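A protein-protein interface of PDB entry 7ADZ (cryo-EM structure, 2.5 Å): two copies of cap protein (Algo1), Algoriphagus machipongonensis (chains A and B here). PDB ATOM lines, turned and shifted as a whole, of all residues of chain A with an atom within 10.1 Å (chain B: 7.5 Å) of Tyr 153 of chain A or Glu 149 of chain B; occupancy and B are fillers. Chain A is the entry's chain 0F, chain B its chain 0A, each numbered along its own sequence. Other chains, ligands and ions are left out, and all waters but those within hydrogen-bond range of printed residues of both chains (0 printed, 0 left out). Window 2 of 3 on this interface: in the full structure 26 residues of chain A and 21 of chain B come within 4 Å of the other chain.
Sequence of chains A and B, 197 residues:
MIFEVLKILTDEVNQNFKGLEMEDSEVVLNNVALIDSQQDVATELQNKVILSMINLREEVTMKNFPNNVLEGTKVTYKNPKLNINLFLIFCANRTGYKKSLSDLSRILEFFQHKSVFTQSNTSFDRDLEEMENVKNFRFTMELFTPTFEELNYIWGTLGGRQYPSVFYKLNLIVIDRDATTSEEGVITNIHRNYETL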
ATOM      1  N   ILE A  54       0.628 -13.115  15.981  1.00  0.00           N
ATOM      2  CA  ILE A  54       1.574 -14.148  16.394  1.00  0.00           C
ATOM      3  C   ILE A  54       2.284 -13.789  17.703  1.00  0.00           C
ATOM      4  O   ILE A  54       2.800 -14.678  18.388  1.00  0.00           O
ATOM      5  CB  ILE A  54       2.571 -14.459  15.258  1.00  0.00           C
ATOM      6  CG1 ILE A  54       3.455 -13.257  14.929  1.00  0.00           C
ATOM      7  CG2 ILE A  54       1.832 -14.942  14.020  1.00  0.00           C
ATOM      8  CD1 ILE A  54       4.356 -13.453  13.737  1.00  0.00           C
ATOM      9  N   ASN A  55       2.327 -12.513  18.093  1.00  0.00           N
ATOM     10  CA  ASN A  55       3.036 -12.140  19.314  1.00  0.00           C
ATOM     11  C   ASN A  55       2.480 -10.841  19.896  1.00  0.00           C
ATOM     12  O   ASN A  55       1.834 -10.053  19.208  1.00  0.00           O
ATOM     13  CB  ASN A  55       4.541 -12.010  19.051  1.00  0.00           C
ATOM     14  CG  ASN A  55       5.371 -12.263  20.285  1.00  0.00           C
ATOM     15  OD1 ASN A  55       4.851 -12.656  21.326  1.00  0.00           O
ATOM     16  ND2 ASN A  55       6.673 -12.047  20.176  1.00  0.00           N
ATOM     17  N   ARG A  57       3.841  -7.596  22.684  1.00  0.00           N
ATOM     18  CA  ARG A  57       4.872  -6.964  23.499  1.00  0.00           C
ATOM     19  C   ARG A  57       4.276  -5.750  24.201  1.00  0.00           C
ATOM     20  O   ARG A  57       3.137  -5.358  23.951  1.00  0.00           O
ATOM     21  CB  ARG A  57       6.096  -6.536  22.672  1.00  0.00           C
ATOM     22  CG  ARG A  57       6.589  -7.540  21.638  1.00  0.00           C
ATOM     23  CD  ARG A  57       7.303  -8.725  22.264  1.00  0.00           C
ATOM     24  NE  ARG A  57       8.728  -8.462  22.417  1.00  0.00           N
ATOM     25  CZ  ARG A  57       9.388  -8.565  23.564  1.00  0.00           C
ATOM     26  NH1 ARG A  57      10.684  -8.297  23.609  1.00  0.00           N
ATOM     27  NH2 ARG A  57       8.759  -8.950  24.660  1.00  0.00           N
ATOM     28  N   PHE A 144       8.436  -5.868   8.516  1.00  0.00           N
ATOM     29  CA  PHE A 144       9.404  -6.597   9.323  1.00  0.00           C
ATOM     30  C   PHE A 144       9.887  -7.816   8.546  1.00  0.00           C
ATOM     31  O   PHE A 144       9.074  -8.622   8.087  1.00  0.00           O
ATOM     32  CB  PHE A 144       8.774  -7.005  10.658  1.00  0.00           C
ATOM     33  CG  PHE A 144       9.523  -8.074  11.383  1.00  0.00           C
ATOM     34  CD1 PHE A 144       8.971  -9.333  11.548  1.00  0.00           C
ATOM     35  CD2 PHE A 144      10.777  -7.824  11.910  1.00  0.00           C
ATOM     36  CE1 PHE A 144       9.657 -10.321  12.212  1.00  0.00           C
ATOM     37  CE2 PHE A 144      11.468  -8.811  12.580  1.00  0.00           C
ATOM     38  CZ  PHE A 144      10.908 -10.061  12.730  1.00  0.00           C
ATOM     39  N   PRO A 146      12.447 -11.102   8.855  1.00  0.00           N
ATOM     40  CA  PRO A 146      13.300 -11.857   9.779  1.00  0.00           C
ATOM     41  C   PRO A 146      14.425 -12.615   9.085  1.00  0.00           C
ATOM     42  O   PRO A 146      14.397 -12.855   7.877  1.00  0.00           O
ATOM     43  CB  PRO A 146      12.312 -12.832  10.428  1.00  0.00           C
ATOM     44  CG  PRO A 146      11.313 -13.087   9.357  1.00  0.00           C
ATOM     45  CD  PRO A 146      11.193 -11.817   8.560  1.00  0.00           C
ATOM     46  N   THR A 147      15.429 -12.996   9.881  1.00  0.00           N
ATOM     47  CA  THR A 147      16.522 -13.835   9.407  1.00  0.00           C
ATOM     48  C   THR A 147      16.097 -15.302   9.369  1.00  0.00           C
ATOM     49  O   THR A 147      14.969 -15.659   9.714  1.00  0.00           O
ATOM     50  CB  THR A 147      17.765 -13.682  10.289  1.00  0.00           C
ATOM     51  OG1 THR A 147      17.507 -14.206  11.596  1.00  0.00           O
ATOM     52  CG2 THR A 147      18.170 -12.231  10.404  1.00  0.00           C
ATOM     53  N   PHE A 148      17.028 -16.160   8.943  1.00  0.00           N
ATOM     54  CA  PHE A 148      16.721 -17.579   8.778  1.00  0.00           C
ATOM     55  C   PHE A 148      16.519 -18.272  10.118  1.00  0.00           C
ATOM     56  O   PHE A 148      15.738 -19.223  10.219  1.00  0.00           O
ATOM     57  CB  PHE A 148      17.825 -18.268   7.978  1.00  0.00           C
ATOM     58  CG  PHE A 148      17.582 -18.272   6.497  1.00  0.00           C
ATOM     59  CD1 PHE A 148      16.331 -18.581   5.991  1.00  0.00           C
ATOM     60  CD2 PHE A 148      18.599 -17.954   5.614  1.00  0.00           C
ATOM     61  CE1 PHE A 148      16.101 -18.576   4.627  1.00  0.00           C
ATOM     62  CE2 PHE A 148      18.377 -17.950   4.252  1.00  0.00           C
ATOM     63  CZ  PHE A 148      17.127 -18.262   3.758  1.00  0.00           C
ATOM     64  N   GLU A 149      17.217 -17.814  11.157  1.00  0.00           N
ATOM     65  CA  GLU A 149      17.022 -18.377  12.486  1.00  0.00           C
ATOM     66  C   GLU A 149      15.667 -17.978  13.063  1.00  0.00           C
ATOM     67  O   GLU A 149      15.026 -18.765  13.768  1.00  0.00           O
ATOM     68  CB  GLU A 149      18.163 -17.941  13.409  1.00  0.00           C
ATOM     69  CG  GLU A 149      18.143 -18.592  14.777  1.00  0.00           C
ATOM     70  CD  GLU A 149      19.154 -17.993  15.730  1.00  0.00           C
ATOM     71  OE1 GLU A 149      18.961 -16.840  16.159  1.00  0.00           O
ATOM     72  OE2 GLU A 149      20.140 -18.681  16.060  1.00  0.00           O
ATOM     73  N   GLU A 150      15.210 -16.759  12.764  1.00  0.00           N
ATOM     74  CA  GLU A 150      13.922 -16.291  13.271  1.00  0.00           C
ATOM     75  C   GLU A 150      12.750 -16.955  12.554  1.00  0.00           C
ATOM     76  O   GLU A 150      11.710 -17.197  13.171  1.00  0.00           O
ATOM     77  CB  GLU A 150      13.829 -14.772  13.149  1.00  0.00           C
ATOM     78  CG  GLU A 150      14.693 -14.001  14.125  1.00  0.00           C
ATOM     79  CD  GLU A 150      14.777 -12.514  13.794  1.00  0.00           C
ATOM     80  OE1 GLU A 150      15.111 -12.171  12.642  1.00  0.00           O
ATOM     81  OE2 GLU A 150      14.505 -11.684  14.684  1.00  0.00           O
ATOM     82  N   LEU A 151      12.884 -17.222  11.247  1.00  0.00           N
ATOM     83  CA  LEU A 151      11.838 -17.940  10.515  1.00  0.00           C
ATOM     84  C   LEU A 151      11.643 -19.353  11.037  1.00  0.00           C
ATOM     85  O   LEU A 151      10.530 -19.887  10.993  1.00  0.00           O
ATOM     86  CB  LEU A 151      12.154 -18.015   9.024  1.00  0.00           C
ATOM     87  CG  LEU A 151      11.877 -16.876   8.063  1.00  0.00           C
ATOM     88  CD1 LEU A 151      12.377 -17.284   6.695  1.00  0.00           C
ATOM     89  CD2 LEU A 151      10.392 -16.616   8.026  1.00  0.00           C
ATOM     90  N   ASN A 152      12.717 -19.979  11.510  1.00  0.00           N
ATOM     91  CA  ASN A 152      12.608 -21.316  12.076  1.00  0.00           C
ATOM     92  C   ASN A 152      11.847 -21.289  13.400  1.00  0.00           C
ATOM     93  O   ASN A 152      11.110 -22.228  13.715  1.00  0.00           O
ATOM     94  CB  ASN A 152      14.008 -21.905  12.238  1.00  0.00           C
ATOM     95  CG  ASN A 152      13.990 -23.358  12.627  1.00  0.00           C
ATOM     96  OD1 ASN A 152      14.228 -23.703  13.781  1.00  0.00           O
ATOM     97  ND2 ASN A 152      13.722 -24.225  11.664  1.00  0.00           N
ATOM     98  N   TYR A 153      12.008 -20.217  14.181  1.00  0.00           N
ATOM     99  CA  TYR A 153      11.255 -20.068  15.424  1.00  0.00           C
ATOM    100  C   TYR A 153       9.773 -19.832  15.161  1.00  0.00           C
ATOM    101  O   TYR A 153       8.919 -20.363  15.878  1.00  0.00           O
ATOM    102  CB  TYR A 153      11.803 -18.903  16.247  1.00  0.00           C
ATOM    103  CG  TYR A 153      13.188 -19.086  16.795  1.00  0.00           C
ATOM    104  CD1 TYR A 153      13.713 -20.350  17.012  1.00  0.00           C
ATOM    105  CD2 TYR A 153      13.963 -17.986  17.127  1.00  0.00           C
ATOM    106  CE1 TYR A 153      14.980 -20.513  17.524  1.00  0.00           C
ATOM    107  CE2 TYR A 153      15.228 -18.137  17.635  1.00  0.00           C
ATOM    108  CZ  TYR A 153      15.731 -19.401  17.834  1.00  0.00           C
ATOM    109  OH  TYR A 153      16.994 -19.555  18.347  1.00  0.00           O
ATOM    110  N   ILE A 154       9.452 -19.018  14.153  1.00  0.00           N
ATOM    111  CA  ILE A 154       8.070 -18.615  13.903  1.00  0.00           C
ATOM    112  C   ILE A 154       7.267 -19.779  13.337  1.00  0.00           C
ATOM    113  O   ILE A 154       6.186 -20.107  13.838  1.00  0.00           O
ATOM    114  CB  ILE A 154       8.036 -17.390  12.974  1.00  0.00           C
ATOM    115  CG1 ILE A 154       8.542 -16.159  13.722  1.00  0.00           C
ATOM    116  CG2 ILE A 154       6.642 -17.157  12.410  1.00  0.00           C
ATOM    117  CD1 ILE A 154       8.755 -14.961  12.855  1.00  0.00           C
ATOM    118  N   TRP A 155       7.785 -20.427  12.292  1.00  0.00           N
ATOM    119  CA  TRP A 155       7.093 -21.563  11.700  1.00  0.00           C
ATOM    120  C   TRP A 155       7.222 -22.830  12.533  1.00  0.00           C
ATOM    121  O   TRP A 155       6.545 -23.818  12.232  1.00  0.00           O
ATOM    122  CB  TRP A 155       7.599 -21.807  10.276  1.00  0.00           C
ATOM    123  CG  TRP A 155       7.035 -20.832   9.292  1.00  0.00           C
ATOM    124  CD1 TRP A 155       7.694 -19.805   8.689  1.00  0.00           C
ATOM    125  CD2 TRP A 155       5.686 -20.775   8.818  1.00  0.00           C
ATOM    126  NE1 TRP A 155       6.844 -19.119   7.867  1.00  0.00           N
ATOM    127  CE2 TRP A 155       5.603 -19.692   7.928  1.00  0.00           C
ATOM    128  CE3 TRP A 155       4.540 -21.539   9.056  1.00  0.00           C
ATOM    129  CZ2 TRP A 155       4.427 -19.353   7.275  1.00  0.00           C
ATOM    130  CZ3 TRP A 155       3.375 -21.199   8.407  1.00  0.00           C
ATOM    131  CH2 TRP A 155       3.326 -20.117   7.528  1.00  0.00           C
ATOM    132  N   GLY A 156       8.069 -22.824  13.563  1.00  0.00           N
ATOM    133  CA  GLY A 156       8.124 -23.947  14.481  1.00  0.00           C
ATOM    134  C   GLY A 156       6.908 -24.032  15.383  1.00  0.00           C
ATOM    135  O   GLY A 156       6.565 -25.108  15.874  1.00  0.00           O
ATOM    136  N   THR A 157       6.250 -22.900  15.626  1.00  0.00           N
ATOM    137  CA  THR A 157       5.026 -22.858  16.418  1.00  0.00           C
ATOM    138  C   THR A 157       3.762 -22.839  15.569  1.00  0.00           C
ATOM    139  O   THR A 157       2.670 -22.693  16.122  1.00  0.00           O
ATOM    140  CB  THR A 157       5.024 -21.636  17.346  1.00  0.00           C
ATOM    141  OG1 THR A 157       4.846 -20.443  16.578  1.00  0.00           O
ATOM    142  CG2 THR A 157       6.326 -21.539  18.117  1.00  0.00           C
ATOM    143  N   LEU A 158       3.876 -22.962  14.250  1.00  0.00           N
ATOM    144  CA  LEU A 158       2.718 -22.947  13.365  1.00  0.00           C
ATOM    145  C   LEU A 158       2.603 -24.217  12.536  1.00  0.00           C
ATOM    146  O   LEU A 158       1.874 -24.226  11.542  1.00  0.00           O
ATOM    147  CB  LEU A 158       2.770 -21.733  12.437  1.00  0.00           C
ATOM    148  CG  LEU A 158       2.821 -20.332  13.048  1.00  0.00           C
ATOM    149  CD1 LEU A 158       3.207 -19.312  11.994  1.00  0.00           C
ATOM    150  CD2 LEU A 158       1.499 -19.971  13.677  1.00  0.00           C
ATOM    151  N   GLY A 159       3.378 -25.254  12.838  1.00  0.00           N
ATOM    152  CA  GLY A 159       3.297 -26.474  12.047  1.00  0.00           C
ATOM    153  C   GLY A 159       4.574 -27.032  11.430  1.00  0.00           C
ATOM    154  O   GLY A 159       4.770 -28.242  11.427  1.00  0.00           O
ATOM    155  N   GLY A 160       5.435 -26.177  10.884  1.00  0.00           N
ATOM    156  CA  GLY A 160       6.683 -26.639  10.292  1.00  0.00           C
ATOM    157  C   GLY A 160       6.717 -26.736   8.776  1.00  0.00           C
ATOM    158  O   GLY A 160       7.641 -27.299   8.195  1.00  0.00           O
ATOM    159  N   PHE A 167       5.435 -10.171   6.932  1.00  0.00           N
ATOM    160  CA  PHE A 167       5.306  -9.901   8.357  1.00  0.00           C
ATOM    161  C   PHE A 167       5.257  -8.400   8.611  1.00  0.00           C
ATOM    162  O   PHE A 167       5.987  -7.635   7.982  1.00  0.00           O
ATOM    163  CB  PHE A 167       6.466 -10.532   9.131  1.00  0.00           C
ATOM    164  CG  PHE A 167       6.483 -12.034   9.082  1.00  0.00           C
ATOM    165  CD1 PHE A 167       5.793 -12.774  10.025  1.00  0.00           C
ATOM    166  CD2 PHE A 167       7.185 -12.707   8.091  1.00  0.00           C
ATOM    167  CE1 PHE A 167       5.805 -14.151   9.991  1.00  0.00           C
ATOM    168  CE2 PHE A 167       7.195 -14.086   8.047  1.00  0.00           C
ATOM    169  CZ  PHE A 167       6.506 -14.809   9.001  1.00  0.00           C
ATOM    170  N   PRO B 146       7.066 -12.780  26.307  1.00  0.00           N
ATOM    171  CA  PRO B 146       8.328 -13.399  25.891  1.00  0.00           C
ATOM    172  C   PRO B 146       8.760 -13.016  24.480  1.00  0.00           C
ATOM    173  O   PRO B 146       7.966 -12.540  23.667  1.00  0.00           O
ATOM    174  CB  PRO B 146       8.010 -14.896  25.970  1.00  0.00           C
ATOM    175  CG  PRO B 146       6.562 -14.965  25.642  1.00  0.00           C
ATOM    176  CD  PRO B 146       5.932 -13.710  26.178  1.00  0.00           C
ATOM    177  N   THR B 147      10.047 -13.236  24.200  1.00  0.00           N
ATOM    178  CA  THR B 147      10.597 -13.044  22.864  1.00  0.00           C
ATOM    179  C   THR B 147      10.277 -14.241  21.973  1.00  0.00           C
ATOM    180  O   THR B 147       9.643 -15.212  22.393  1.00  0.00           O
ATOM    181  CB  THR B 147      12.112 -12.827  22.911  1.00  0.00           C
ATOM    182  OG1 THR B 147      12.766 -14.021  23.353  1.00  0.00           O
ATOM    183  CG2 THR B 147      12.467 -11.690  23.841  1.00  0.00           C
ATOM    184  N   PHE B 148      10.734 -14.164  20.720  1.00  0.00           N
ATOM    185  CA  PHE B 148      10.421 -15.205  19.743  1.00  0.00           C
ATOM    186  C   PHE B 148      11.143 -16.508  20.056  1.00  0.00           C
ATOM    187  O   PHE B 148      10.629 -17.593  19.766  1.00  0.00           O
ATOM    188  CB  PHE B 148      10.766 -14.726  18.334  1.00  0.00           C
ATOM    189  CG  PHE B 148       9.628 -14.040  17.636  1.00  0.00           C
ATOM    190  CD1 PHE B 148       8.351 -14.573  17.684  1.00  0.00           C
ATOM    191  CD2 PHE B 148       9.831 -12.859  16.945  1.00  0.00           C
ATOM    192  CE1 PHE B 148       7.297 -13.940  17.050  1.00  0.00           C
ATOM    193  CE2 PHE B 148       8.785 -12.223  16.308  1.00  0.00           C
ATOM    194  CZ  PHE B 148       7.516 -12.764  16.359  1.00  0.00           C
ATOM    195  N   GLU B 149      12.336 -16.423  20.644  1.00  0.00           N
ATOM    196  CA  GLU B 149      13.052 -17.627  21.043  1.00  0.00           C
ATOM    197  C   GLU B 149      12.377 -18.304  22.233  1.00  0.00           C
ATOM    198  O   GLU B 149      12.357 -19.537  22.326  1.00  0.00           O
ATOM    199  CB  GLU B 149      14.510 -17.283  21.358  1.00  0.00           C
ATOM    200  CG  GLU B 149      15.388 -18.485  21.639  1.00  0.00           C
ATOM    201  CD  GLU B 149      16.762 -18.109  22.145  1.00  0.00           C
ATOM    202  OE1 GLU B 149      16.867 -17.632  23.291  1.00  0.00           O
ATOM    203  OE2 GLU B 149      17.744 -18.297  21.400  1.00  0.00           O
ATOM    204  N   GLU B 150      11.811 -17.513  23.147  1.00  0.00           N
ATOM    205  CA  GLU B 150      11.142 -18.074  24.318  1.00  0.00           C
ATOM    206  C   GLU B 150       9.797 -18.702  23.962  1.00  0.00           C
ATOM    207  O   GLU B 150       9.402 -19.698  24.575  1.00  0.00           O
ATOM    208  CB  GLU B 150      10.960 -16.998  25.386  1.00  0.00           C
ATOM    209  CG  GLU B 150      12.233 -16.583  26.093  1.00  0.00           C
ATOM    210  CD  GLU B 150      12.055 -15.332  26.947  1.00  0.00           C
ATOM    211  OE1 GLU B 150      11.563 -14.311  26.426  1.00  0.00           O
ATOM    212  OE2 GLU B 150      12.402 -15.369  28.145  1.00  0.00           O
ATOM    213  N   LEU B 151       9.064 -18.115  23.005  1.00  0.00           N
ATOM    214  CA  LEU B 151       7.808 -18.712  22.546  1.00  0.00           C
ATOM    215  C   LEU B 151       8.022 -20.068  21.897  1.00  0.00           C
ATOM    216  O   LEU B 151       7.153 -20.942  21.973  1.00  0.00           O
ATOM    217  CB  LEU B 151       7.093 -17.807  21.549  1.00  0.00           C
ATOM    218  CG  LEU B 151       6.239 -16.627  21.968  1.00  0.00           C
ATOM    219  CD1 LEU B 151       5.751 -15.930  20.718  1.00  0.00           C
ATOM    220  CD2 LEU B 151       5.072 -17.128  22.782  1.00  0.00           C
ATOM    221  N   ASN B 152       9.162 -20.250  21.235  1.00  0.00           N
ATOM    222  CA  ASN B 152       9.469 -21.535  20.626  1.00  0.00           C
ATOM    223  C   ASN B 152       9.738 -22.596  21.693  1.00  0.00           C
ATOM    224  O   ASN B 152       9.395 -23.767  21.508  1.00  0.00           O
ATOM    225  CB  ASN B 152      10.657 -21.369  19.680  1.00  0.00           C
ATOM    226  CG  ASN B 152      10.923 -22.596  18.852  1.00  0.00           C
ATOM    227  OD1 ASN B 152      11.854 -23.348  19.124  1.00  0.00           O
ATOM    228  ND2 ASN B 152      10.116 -22.802  17.823  1.00  0.00           N
ATOM    229  N   TYR B 153      10.342 -22.198  22.816  1.00  0.00           N
ATOM    230  CA  TYR B 153      10.562 -23.126  23.924  1.00  0.00           C
ATOM    231  C   TYR B 153       9.253 -23.524  24.595  1.00  0.00           C
ATOM    232  O   TYR B 153       9.072 -24.686  24.973  1.00  0.00           O
ATOM    233  CB  TYR B 153      11.488 -22.506  24.969  1.00  0.00           C
ATOM    234  CG  TYR B 153      12.904 -22.274  24.531  1.00  0.00           C
ATOM    235  CD1 TYR B 153      13.470 -23.019  23.509  1.00  0.00           C
ATOM    236  CD2 TYR B 153      13.687 -21.323  25.164  1.00  0.00           C
ATOM    237  CE1 TYR B 153      14.773 -22.808  23.117  1.00  0.00           C
ATOM    238  CE2 TYR B 153      14.986 -21.103  24.779  1.00  0.00           C
ATOM    239  CZ  TYR B 153      15.525 -21.849  23.758  1.00  0.00           C
ATOM    240  OH  TYR B 153      16.824 -21.636  23.375  1.00  0.00           O
ATOM    241  N   ILE B 154       8.343 -22.563  24.777  1.00  0.00           N
ATOM    242  CA  ILE B 154       7.116 -22.803  25.532  1.00  0.00           C
ATOM    243  C   ILE B 154       6.161 -23.684  24.738  1.00  0.00           C
ATOM    244  O   ILE B 154       5.662 -24.697  25.242  1.00  0.00           O
ATOM    245  CB  ILE B 154       6.467 -21.465  25.927  1.00  0.00           C
ATOM    246  CG1 ILE B 154       7.310 -20.777  26.997  1.00  0.00           C
ATOM    247  CG2 ILE B 154       5.033 -21.659  26.396  1.00  0.00           C
ATOM    248  CD1 ILE B 154       6.891 -19.376  27.298  1.00  0.00           C
ATOM    249  N   GLN B 162       0.379 -23.065  18.128  1.00  0.00           N
ATOM    250  CA  GLN B 162       0.013 -22.063  19.113  1.00  0.00           C
ATOM    251  C   GLN B 162      -1.452 -21.649  18.978  1.00  0.00           C
ATOM    252  O   GLN B 162      -2.139 -21.975  18.010  1.00  0.00           O
ATOM    253  CB  GLN B 162       0.920 -20.837  18.992  1.00  0.00           C
ATOM    254  CG  GLN B 162       0.538 -19.868  17.899  1.00  0.00           C
ATOM    255  CD  GLN B 162       1.285 -18.557  18.004  1.00  0.00           C
ATOM    256  OE1 GLN B 162       0.834 -17.625  18.664  1.00  0.00           O
ATOM    257  NE2 GLN B 162       2.433 -18.474  17.347  1.00  0.00           N
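The backbone NH (N) of Thr 147 of chain B lies within hydrogen-bond range of the side-chain carboxylate (OE1) of Glu 150 of chain B (2.9 Å). O of Ile 154 of chain A is in hydrogen-bond range of OG1 of Thr 157 of chain A, at 3.1 Å.
Of chain B, only Phe 148, Glu 149 and Asn 152 come within 4 Å of Tyr 153 of chain A. Of chain A, only Tyr 153 comes within 4 Å of Glu 149 of chain B. Thr 147 of chain B touches just one residue of chain A: Arg 57 (3.8 Å). Printed residues of chain A within 4 Å of Leu 151 of chain B: Ile 54, Asn 55 and Thr 157. Printed residues of chain B within 4 Å of Arg 57 of chain A: Pro 146 and Thr 147. Of the printed residues of chain B, Thr 157 of chain A touches Leu 151 (3.99 Å) and Gln 162 (3.1 Å). Of the printed residues of chain A, Gln 162 of chain B touches Ile 54 (3.6 Å) and Thr 157 (3.1 Å). Printed residues of chain A within 4 Å of Phe 148 of chain B: Asn 55 and Tyr 153. The nearest residue of chain A that does not touch Glu 149 of chain B is Glu 149 of chain A (5.6 Å). The nearest printed residue of chain B that does not touch Arg 57 of chain A is Phe 148 of chain B (6.3 Å).
Among the printed residues, pairs that only touch across the chains: Ile 54 of chain A with Leu 151 of chain B, Ile 54 of chain A with Gln 162 of chain B, Asn 55 of chain A with Pro 146 of chain B, Asn 55 of chain A with Phe 148 of chain B, Asn 55 of chain A with Leu 151 of chain B, Arg 57 of chain A with Pro 146 of chain B, Arg 57 of chain A with Thr 147 of chain B, Tyr 153 of chain A with Phe 148 of chain B and Thr 157 of chain A with Leu 151 of chain B.
Tyr 153 of chain A touches Phe 148 of chain B, but with the chains exchanged Phe 148 of chain A does not touch Tyr 153 of chain B (13.4 Å). Tyr 153 of chain A touches Glu 149 of chain B, but with the chains exchanged Glu 149 of chain A does not touch Tyr 153 of chain B (8.6 Å). Tyr 153 of chain A touches Asn 152 of chain B, but with the chains exchanged Asn 152 of chain A does not touch Tyr 153 of chain B (9.1 Å). Positions printed for both chains: 146, 147, 148, 149, 150, 151, 152, 153 and 154. Of the 12 pairs that touch across the chains among the printed residues, none has its exchanged pair printed and touching as well.
The side-chain carboxylate of Glu 149 of chain B sits at hydrogen-bond distance from the side-chain hydroxyl of Tyr 153 of chain A, at 3.4 Å. ND2 of Asn 152 of chain B lies within hydrogen-bond range of O of Tyr 153 of chain A (3.3 Å). N of Gln 162 of chain B is in hydrogen-bond range of O of Thr 157 of chain A (3.1 Å).
Printed residues of chain B that touch a printed residue of chain A: Pro 146, Thr 147, Phe 148, Glu 149, Leu 151, Asn 152 and Gln 162. Hydrophobic or aromatic side chains of chain A that line the printed part of chain B: Tyr 153. Among the printed residues, no Asp or Glu carboxylate lies within 4 Å of a Lys or Arg side-chain nitrogen of the other chain.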
